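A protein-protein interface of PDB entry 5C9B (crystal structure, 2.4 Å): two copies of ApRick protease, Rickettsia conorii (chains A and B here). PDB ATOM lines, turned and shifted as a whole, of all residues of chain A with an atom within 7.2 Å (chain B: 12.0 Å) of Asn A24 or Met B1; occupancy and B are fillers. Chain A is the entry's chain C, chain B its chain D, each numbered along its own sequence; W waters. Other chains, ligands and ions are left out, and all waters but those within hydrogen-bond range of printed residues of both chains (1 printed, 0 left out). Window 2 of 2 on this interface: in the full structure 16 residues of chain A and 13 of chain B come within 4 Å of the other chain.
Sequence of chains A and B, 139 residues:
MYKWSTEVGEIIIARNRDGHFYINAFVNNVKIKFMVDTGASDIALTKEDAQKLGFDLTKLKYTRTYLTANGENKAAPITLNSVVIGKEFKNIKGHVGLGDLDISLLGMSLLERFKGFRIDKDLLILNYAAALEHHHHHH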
ATOM      1  N   GLU A  10     -27.886  -3.504 -14.181  1.00  0.00           N
ATOM      2  CA  GLU A  10     -26.660  -4.273 -14.304  1.00  0.00           C
ATOM      3  C   GLU A  10     -25.520  -3.324 -14.610  1.00  0.00           C
ATOM      4  O   GLU A  10     -25.615  -2.497 -15.525  1.00  0.00           O
ATOM      5  CB  GLU A  10     -26.741  -5.286 -15.447  1.00  0.00           C
ATOM      6  CG  GLU A  10     -25.573  -6.276 -15.459  1.00  0.00           C
ATOM      7  CD  GLU A  10     -25.826  -7.557 -16.279  1.00  0.00           C
ATOM      8  OE1 GLU A  10     -25.982  -7.464 -17.504  1.00  0.00           O
ATOM      9  OE2 GLU A  10     -25.818  -8.670 -15.709  1.00  0.00           O
ATOM     10  N   ILE A  11     -24.425  -3.498 -13.894  1.00  0.00           N
ATOM     11  CA  ILE A  11     -23.217  -2.783 -14.214  1.00  0.00           C
ATOM     12  C   ILE A  11     -22.099  -3.797 -14.473  1.00  0.00           C
ATOM     13  O   ILE A  11     -21.845  -4.677 -13.663  1.00  0.00           O
ATOM     14  CB  ILE A  11     -22.870  -1.864 -13.043  1.00  0.00           C
ATOM     15  CG1 ILE A  11     -23.830  -0.693 -13.030  1.00  0.00           C
ATOM     16  CG2 ILE A  11     -21.438  -1.389 -13.104  1.00  0.00           C
ATOM     17  CD1 ILE A  11     -23.775   0.085 -11.732  1.00  0.00           C
ATOM     18  N   ILE A  12     -21.412  -3.664 -15.592  1.00  0.00           N
ATOM     19  CA  ILE A  12     -20.250  -4.507 -15.851  1.00  0.00           C
ATOM     20  C   ILE A  12     -18.985  -3.624 -15.924  1.00  0.00           C
ATOM     21  O   ILE A  12     -18.985  -2.570 -16.532  1.00  0.00           O
ATOM     22  CB  ILE A  12     -20.429  -5.221 -17.154  1.00  0.00           C
ATOM     23  CG1 ILE A  12     -21.678  -6.088 -17.084  1.00  0.00           C
ATOM     24  CG2 ILE A  12     -19.241  -6.128 -17.430  1.00  0.00           C
ATOM     25  CD1 ILE A  12     -21.967  -6.807 -18.361  1.00  0.00           C
ATOM     26  N   ILE A  13     -17.916  -4.060 -15.277  1.00  0.00           N
ATOM     27  CA  ILE A  13     -16.657  -3.386 -15.354  1.00  0.00           C
ATOM     28  C   ILE A  13     -15.663  -4.394 -15.886  1.00  0.00           C
ATOM     29  O   ILE A  13     -15.584  -5.524 -15.413  1.00  0.00           O
ATOM     30  CB  ILE A  13     -16.178  -2.942 -13.979  1.00  0.00           C
ATOM     31  CG1 ILE A  13     -17.280  -2.235 -13.220  1.00  0.00           C
ATOM     32  CG2 ILE A  13     -14.964  -2.037 -14.082  1.00  0.00           C
ATOM     33  CD1 ILE A  13     -17.769  -0.987 -13.883  1.00  0.00           C
ATOM     34  N   ALA A  14     -14.905  -3.988 -16.880  1.00  0.00           N
ATOM     35  CA  ALA A  14     -13.838  -4.831 -17.392  1.00  0.00           C
ATOM     36  C   ALA A  14     -12.538  -4.498 -16.706  1.00  0.00           C
ATOM     37  O   ALA A  14     -12.349  -3.386 -16.204  1.00  0.00           O
ATOM     38  CB  ALA A  14     -13.703  -4.621 -18.862  1.00  0.00           C
ATOM     39  N   TYR A  22     -11.775  -0.648 -11.600  1.00  0.00           N
ATOM     40  CA  TYR A  22     -11.930   0.723 -11.129  1.00  0.00           C
ATOM     41  C   TYR A  22     -13.385   1.082 -11.285  1.00  0.00           C
ATOM     42  O   TYR A  22     -14.022   0.682 -12.232  1.00  0.00           O
ATOM     43  CB  TYR A  22     -11.125   1.681 -12.012  1.00  0.00           C
ATOM     44  CG  TYR A  22      -9.648   1.522 -11.816  1.00  0.00           C
ATOM     45  CD1 TYR A  22      -8.963   0.573 -12.519  1.00  0.00           C
ATOM     46  CD2 TYR A  22      -8.953   2.259 -10.851  1.00  0.00           C
ATOM     47  CE1 TYR A  22      -7.604   0.363 -12.327  1.00  0.00           C
ATOM     48  CE2 TYR A  22      -7.589   2.058 -10.656  1.00  0.00           C
ATOM     49  CZ  TYR A  22      -6.925   1.091 -11.397  1.00  0.00           C
ATOM     50  OH  TYR A  22      -5.593   0.850 -11.266  1.00  0.00           O
ATOM     51  N   ILE A  23     -13.919   1.869 -10.381  1.00  0.00           N
ATOM     52  CA  ILE A  23     -15.332   2.114 -10.414  1.00  0.00           C
ATOM     53  C   ILE A  23     -15.645   3.445  -9.785  1.00  0.00           C
ATOM     54  O   ILE A  23     -15.030   3.828  -8.794  1.00  0.00           O
ATOM     55  CB  ILE A  23     -16.037   0.974  -9.699  1.00  0.00           C
ATOM     56  CG1 ILE A  23     -17.534   0.989  -9.945  1.00  0.00           C
ATOM     57  CG2 ILE A  23     -15.789   1.007  -8.218  1.00  0.00           C
ATOM     58  CD1 ILE A  23     -18.150  -0.286  -9.422  1.00  0.00           C
ATOM     59  N   ASN A  24     -16.582   4.170 -10.373  1.00  0.00           N
ATOM     60  CA  ASN A  24     -16.973   5.462  -9.798  1.00  0.00           C
ATOM     61  C   ASN A  24     -18.186   5.321  -8.923  1.00  0.00           C
ATOM     62  O   ASN A  24     -19.127   4.658  -9.299  1.00  0.00           O
ATOM     63  CB  ASN A  24     -17.275   6.459 -10.890  1.00  0.00           C
ATOM     64  CG  ASN A  24     -16.057   6.767 -11.722  1.00  0.00           C
ATOM     65  OD1 ASN A  24     -14.970   6.963 -11.188  1.00  0.00           O
ATOM     66  ND2 ASN A  24     -16.214   6.745 -13.033  1.00  0.00           N
ATOM     67  N   ALA A  25     -18.164   5.967  -7.761  1.00  0.00           N
ATOM     68  CA  ALA A  25     -19.328   6.043  -6.925  1.00  0.00           C
ATOM     69  C   ALA A  25     -19.614   7.477  -6.558  1.00  0.00           C
ATOM     70  O   ALA A  25     -18.741   8.333  -6.626  1.00  0.00           O
ATOM     71  CB  ALA A  25     -19.094   5.248  -5.657  1.00  0.00           C
ATOM     72  N   PHE A  26     -20.838   7.724  -6.121  1.00  0.00           N
ATOM     73  CA  PHE A  26     -21.148   8.965  -5.430  1.00  0.00           C
ATOM     74  C   PHE A  26     -21.260   8.583  -3.979  1.00  0.00           C
ATOM     75  O   PHE A  26     -21.988   7.661  -3.597  1.00  0.00           O
ATOM     76  CB  PHE A  26     -22.460   9.602  -5.926  1.00  0.00           C
ATOM     77  CG  PHE A  26     -22.410  10.084  -7.362  1.00  0.00           C
ATOM     78  CD1 PHE A  26     -21.699  11.216  -7.696  1.00  0.00           C
ATOM     79  CD2 PHE A  26     -23.040   9.381  -8.365  1.00  0.00           C
ATOM     80  CE1 PHE A  26     -21.634  11.656  -8.992  1.00  0.00           C
ATOM     81  CE2 PHE A  26     -22.976   9.814  -9.669  1.00  0.00           C
ATOM     82  CZ  PHE A  26     -22.278  10.961  -9.979  1.00  0.00           C
ATOM     83  N   LYS A  31     -18.575  12.699  -6.166  1.00  0.00           N
ATOM     84  CA  LYS A  31     -17.997  11.731  -7.080  1.00  0.00           C
ATOM     85  C   LYS A  31     -16.672  11.322  -6.454  1.00  0.00           C
ATOM     86  O   LYS A  31     -15.887  12.185  -6.066  1.00  0.00           O
ATOM     87  CB  LYS A  31     -17.811  12.337  -8.483  1.00  0.00           C
ATOM     88  CG  LYS A  31     -16.870  11.558  -9.412  1.00  0.00           C
ATOM     89  CD  LYS A  31     -17.587  10.826 -10.533  1.00  0.00           C
ATOM     90  CE  LYS A  31     -18.668   9.891 -10.004  1.00  0.00           C
ATOM     91  NZ  LYS A  31     -19.460   9.302 -11.120  1.00  0.00           N
ATOM     92  N   ILE A  32     -16.487  10.006  -6.287  1.00  0.00           N
ATOM     93  CA  ILE A  32     -15.253   9.418  -5.836  1.00  0.00           C
ATOM     94  C   ILE A  32     -14.863   8.251  -6.740  1.00  0.00           C
ATOM     95  O   ILE A  32     -15.699   7.378  -7.050  1.00  0.00           O
ATOM     96  CB  ILE A  32     -15.362   8.827  -4.439  1.00  0.00           C
ATOM     97  CG1 ILE A  32     -15.874   9.860  -3.452  1.00  0.00           C
ATOM     98  CG2 ILE A  32     -13.990   8.355  -3.987  1.00  0.00           C
ATOM     99  CD1 ILE A  32     -14.839  10.908  -3.107  1.00  0.00           C
ATOM    100  N   LYS A  33     -13.581   8.231  -7.105  1.00  0.00           N
ATOM    101  CA  LYS A  33     -12.997   7.173  -7.903  1.00  0.00           C
ATOM    102  C   LYS A  33     -12.445   6.135  -6.973  1.00  0.00           C
ATOM    103  O   LYS A  33     -11.684   6.472  -6.060  1.00  0.00           O
ATOM    104  CB  LYS A  33     -11.862   7.722  -8.757  1.00  0.00           C
ATOM    105  CG  LYS A  33     -12.328   8.618  -9.895  1.00  0.00           C
ATOM    106  CD  LYS A  33     -11.525   8.391 -11.172  1.00  0.00           C
ATOM    107  CE  LYS A  33     -11.661   6.961 -11.704  1.00  0.00           C
ATOM    108  NZ  LYS A  33     -12.119   6.959 -13.121  1.00  0.00           N
ATOM    109  N   PHE A  34     -12.845   4.885  -7.193  1.00  0.00           N
ATOM    110  CA  PHE A  34     -12.395   3.761  -6.394  1.00  0.00           C
ATOM    111  C   PHE A  34     -11.686   2.761  -7.248  1.00  0.00           C
ATOM    112  O   PHE A  34     -11.971   2.650  -8.427  1.00  0.00           O
ATOM    113  CB  PHE A  34     -13.579   3.032  -5.768  1.00  0.00           C
ATOM    114  CG  PHE A  34     -14.180   3.754  -4.610  1.00  0.00           C
ATOM    115  CD1 PHE A  34     -13.537   3.757  -3.380  1.00  0.00           C
ATOM    116  CD2 PHE A  34     -15.335   4.437  -4.751  1.00  0.00           C
ATOM    117  CE1 PHE A  34     -14.051   4.411  -2.300  1.00  0.00           C
ATOM    118  CE2 PHE A  34     -15.875   5.097  -3.671  1.00  0.00           C
ATOM    119  CZ  PHE A  34     -15.230   5.085  -2.444  1.00  0.00           C
ATOM    120  N   VAL A  84     -23.761   5.598  -3.660  1.00  0.00           N
ATOM    121  CA  VAL A  84     -24.510   5.218  -4.845  1.00  0.00           C
ATOM    122  C   VAL A  84     -23.641   4.651  -5.929  1.00  0.00           C
ATOM    123  O   VAL A  84     -22.725   5.318  -6.391  1.00  0.00           O
ATOM    124  CB  VAL A  84     -25.199   6.440  -5.445  1.00  0.00           C
ATOM    125  CG1 VAL A  84     -25.969   6.056  -6.710  1.00  0.00           C
ATOM    126  CG2 VAL A  84     -26.059   7.084  -4.380  1.00  0.00           C
ATOM    127  N   ILE A  85     -23.956   3.419  -6.325  1.00  0.00           N
ATOM    128  CA  ILE A  85     -23.407   2.765  -7.493  1.00  0.00           C
ATOM    129  C   ILE A  85     -24.582   1.948  -8.045  1.00  0.00           C
ATOM    130  O   ILE A  85     -24.853   0.829  -7.602  1.00  0.00           O
ATOM    131  CB  ILE A  85     -22.295   1.747  -7.141  1.00  0.00           C
ATOM    132  CG1 ILE A  85     -21.190   2.363  -6.309  1.00  0.00           C
ATOM    133  CG2 ILE A  85     -21.768   1.099  -8.419  1.00  0.00           C
ATOM    134  CD1 ILE A  85     -20.076   1.409  -5.910  1.00  0.00           C
ATOM    135  N   GLY A  86     -25.266   2.501  -9.023  1.00  0.00           N
ATOM    136  CA  GLY A  86     -26.517   1.941  -9.497  1.00  0.00           C
ATOM    137  C   GLY A  86     -27.657   2.409  -8.611  1.00  0.00           C
ATOM    138  O   GLY A  86     -28.468   3.205  -9.031  1.00  0.00           O
ATOM    139  N   LEU A 106     -12.362  -0.018  -2.665  1.00  0.00           N
ATOM    140  CA  LEU A 106     -13.690  -0.524  -2.369  1.00  0.00           C
ATOM    141  C   LEU A 106     -13.565  -2.026  -2.085  1.00  0.00           C
ATOM    142  O   LEU A 106     -13.005  -2.768  -2.877  1.00  0.00           O
ATOM    143  CB  LEU A 106     -14.567  -0.269  -3.564  1.00  0.00           C
ATOM    144  CG  LEU A 106     -16.021  -0.688  -3.545  1.00  0.00           C
ATOM    145  CD1 LEU A 106     -16.759  -0.037  -2.416  1.00  0.00           C
ATOM    146  CD2 LEU A 106     -16.642  -0.275  -4.860  1.00  0.00           C
ATOM    147  N   MET B   1     -17.058   1.045 -18.232  1.00  0.00           N
ATOM    148  CA  MET B   1     -18.287   0.771 -17.457  1.00  0.00           C
ATOM    149  C   MET B   1     -19.395   0.594 -18.438  1.00  0.00           C
ATOM    150  O   MET B   1     -19.746   1.518 -19.180  1.00  0.00           O
ATOM    151  CB  MET B   1     -18.669   1.861 -16.488  1.00  0.00           C
ATOM    152  CG  MET B   1     -19.875   1.408 -15.693  1.00  0.00           C
ATOM    153  SD  MET B   1     -20.427   2.695 -14.315  1.00  0.00           S
ATOM    154  CE  MET B   1     -18.990   2.660 -12.931  1.00  0.00           C
ATOM    155  N   TYR B   2     -19.964  -0.606 -18.431  1.00  0.00           N
ATOM    156  CA  TYR B   2     -21.208  -0.858 -19.151  1.00  0.00           C
ATOM    157  C   TYR B   2     -22.328  -0.875 -18.131  1.00  0.00           C
ATOM    158  O   TYR B   2     -22.231  -1.542 -17.114  1.00  0.00           O
ATOM    159  CB  TYR B   2     -21.166  -2.190 -19.831  1.00  0.00           C
ATOM    160  CG  TYR B   2     -19.865  -2.538 -20.463  1.00  0.00           C
ATOM    161  CD1 TYR B   2     -18.788  -2.905 -19.705  1.00  0.00           C
ATOM    162  CD2 TYR B   2     -19.731  -2.562 -21.817  1.00  0.00           C
ATOM    163  CE1 TYR B   2     -17.602  -3.262 -20.281  1.00  0.00           C
ATOM    164  CE2 TYR B   2     -18.551  -2.920 -22.407  1.00  0.00           C
ATOM    165  CZ  TYR B   2     -17.484  -3.279 -21.635  1.00  0.00           C
ATOM    166  OH  TYR B   2     -16.286  -3.673 -22.227  1.00  0.00           O
ATOM    167  N   LYS B   3     -23.364  -0.112 -18.388  1.00  0.00           N
ATOM    168  CA  LYS B   3     -24.366   0.163 -17.394  1.00  0.00           C
ATOM    169  C   LYS B   3     -25.694   0.041 -18.081  1.00  0.00           C
ATOM    170  O   LYS B   3     -25.876   0.599 -19.135  1.00  0.00           O
ATOM    171  CB  LYS B   3     -24.238   1.575 -16.828  1.00  0.00           C
ATOM    172  CG  LYS B   3     -25.343   1.864 -15.807  1.00  0.00           C
ATOM    173  CD  LYS B   3     -25.041   2.991 -14.826  1.00  0.00           C
ATOM    174  CE  LYS B   3     -26.207   3.170 -13.852  1.00  0.00           C
ATOM    175  NZ  LYS B   3     -26.204   4.499 -13.167  1.00  0.00           N
ATOM    176  N   TRP B   4     -26.641  -0.666 -17.478  1.00  0.00           N
ATOM    177  CA  TRP B   4     -27.881  -0.934 -18.145  1.00  0.00           C
ATOM    178  C   TRP B   4     -28.996  -0.830 -17.099  1.00  0.00           C
ATOM    179  O   TRP B   4     -28.812  -1.279 -15.977  1.00  0.00           O
ATOM    180  CB  TRP B   4     -27.768  -2.351 -18.860  1.00  0.00           C
ATOM    181  CG  TRP B   4     -29.075  -2.856 -19.410  1.00  0.00           C
ATOM    182  CD1 TRP B   4     -29.672  -2.482 -20.588  1.00  0.00           C
ATOM    183  CD2 TRP B   4     -30.004  -3.747 -18.761  1.00  0.00           C
ATOM    184  NE1 TRP B   4     -30.902  -3.103 -20.717  1.00  0.00           N
ATOM    185  CE2 TRP B   4     -31.127  -3.878 -19.607  1.00  0.00           C
ATOM    186  CE3 TRP B   4     -30.006  -4.431 -17.535  1.00  0.00           C
ATOM    187  CZ2 TRP B   4     -32.221  -4.691 -19.278  1.00  0.00           C
ATOM    188  CZ3 TRP B   4     -31.096  -5.249 -17.215  1.00  0.00           C
ATOM    189  CH2 TRP B   4     -32.183  -5.364 -18.079  1.00  0.00           C
ATOM    190  N   SER B   5     -30.150  -0.246 -17.436  1.00  0.00           N
ATOM    191  CA  SER B   5     -31.330  -0.433 -16.563  1.00  0.00           C
ATOM    192  C   SER B   5     -32.752  -0.473 -17.197  1.00  0.00           C
ATOM    193  O   SER B   5     -32.948  -0.108 -18.336  1.00  0.00           O
ATOM    194  CB  SER B   5     -31.282   0.635 -15.534  1.00  0.00           C
ATOM    195  OG  SER B   5     -31.177   1.804 -16.275  1.00  0.00           O
HETATM  196  O   HOH W   1     -15.175  -1.003 -18.043  1.00  0.00           O
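The backbone carbonyl oxygen (O) of Glu A10 sits at hydrogen-bond distance from the backbone NH (N) of Trp B4 (2.9 Å).
O of Tyr B2 lies within hydrogen-bond range of N of Ile A12 (2.7 Å).
The backbone NH (N) of Ile A23 is in hydrogen-bond range of the backbone carbonyl oxygen (O) of Phe A34, at 2.9 Å.
The side-chain amide oxygen of Asn A24 lies close to the side-chain amino group of Lys A33 (3.4 Å).
Glu A10 touches Tyr B2 (O to O, 3.9 Å).
O of Glu A10 touches CA of Lys B3 (3.5 Å).
Ile A11 touches Tyr B2 (CA to O, 3.3 Å).
Ile A12 touches Met B1.
Ile A13 touches Met B1 (CD1 to CG, 3.7 Å).
Ile A23 touches Met B1.
N of Asn A24 touches CE of Met B1, at 3.8 Å.
Of the printed residues of chain B, Glu A10 touches Tyr B2 (3.9 Å), Lys B3 (3.5 Å) and Trp B4 (2.9 Å).
Of chain B, only Tyr B2 (3.3 Å) comes within 4 Å of Ile A11.
No residue of chain B comes within 4 Å of Ala A14.
Tyr A22 touches none of the printed residues of chain B.
Asn A24 touches just one residue of chain B: Met B1.
No residue of chain B comes within 4 Å of Phe A26.
No residue of chain B comes within 4 Å of Lys A31.
No residue of chain B comes within 4 Å of Phe A34.
Leu A106 touches none of the printed residues of chain B.
Printed residues of chain A within 4 Å of Met B1: Ile A12, Ile A13, Ile A23 and Asn A24.
Of the printed residues of chain A, Tyr B2 touches Glu A10 (3.9 Å), Ile A11 (3.3 Å) and Ile A12 (2.7 Å).
Printed residues of chain A within 4 Å of Lys B3: Glu A10 (3.5 Å).
Of the printed residues of chain A, Trp B4 touches Glu A10.
The nearest residue of chain B that does not touch Asn A24 is Lys B3 (8.1 Å).
The nearest residue of chain A that does not touch Met B1 is Ile A11 (4.1 Å).
The nearest printed residue of chain A that does not touch Lys B3 is Ile A11 (4.1 Å).
Hydrophobic or aromatic side chains of chain B that line the printed part of chain A: Met B1, Tyr B2 and Trp B4.
Of the 18 printed residues of chain A, 6 touch a printed residue of chain B.
Printed residues of chain A that touch a printed residue of chain B: Glu A10, Ile A11, Ile A12, Ile A13, Ile A23 and Asn A24.
Hydrophobic or aromatic side chains of chain A that line the printed part of chain B: Ile A12, Ile A13 and Ile A23.
Among the printed residues, 9 pairs touch across the chains.
Among the printed residues, no Asp or Glu carboxylate lies within 4 Å of a Lys or Arg side-chain nitrogen of the other chain.
No position is printed for both chains.
Water W1 lies within hydrogen-bond range of the backbone NH (N) of Met B1 (2.8 Å) and the backbone NH (N) of Ala A14 (3.2 Å).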
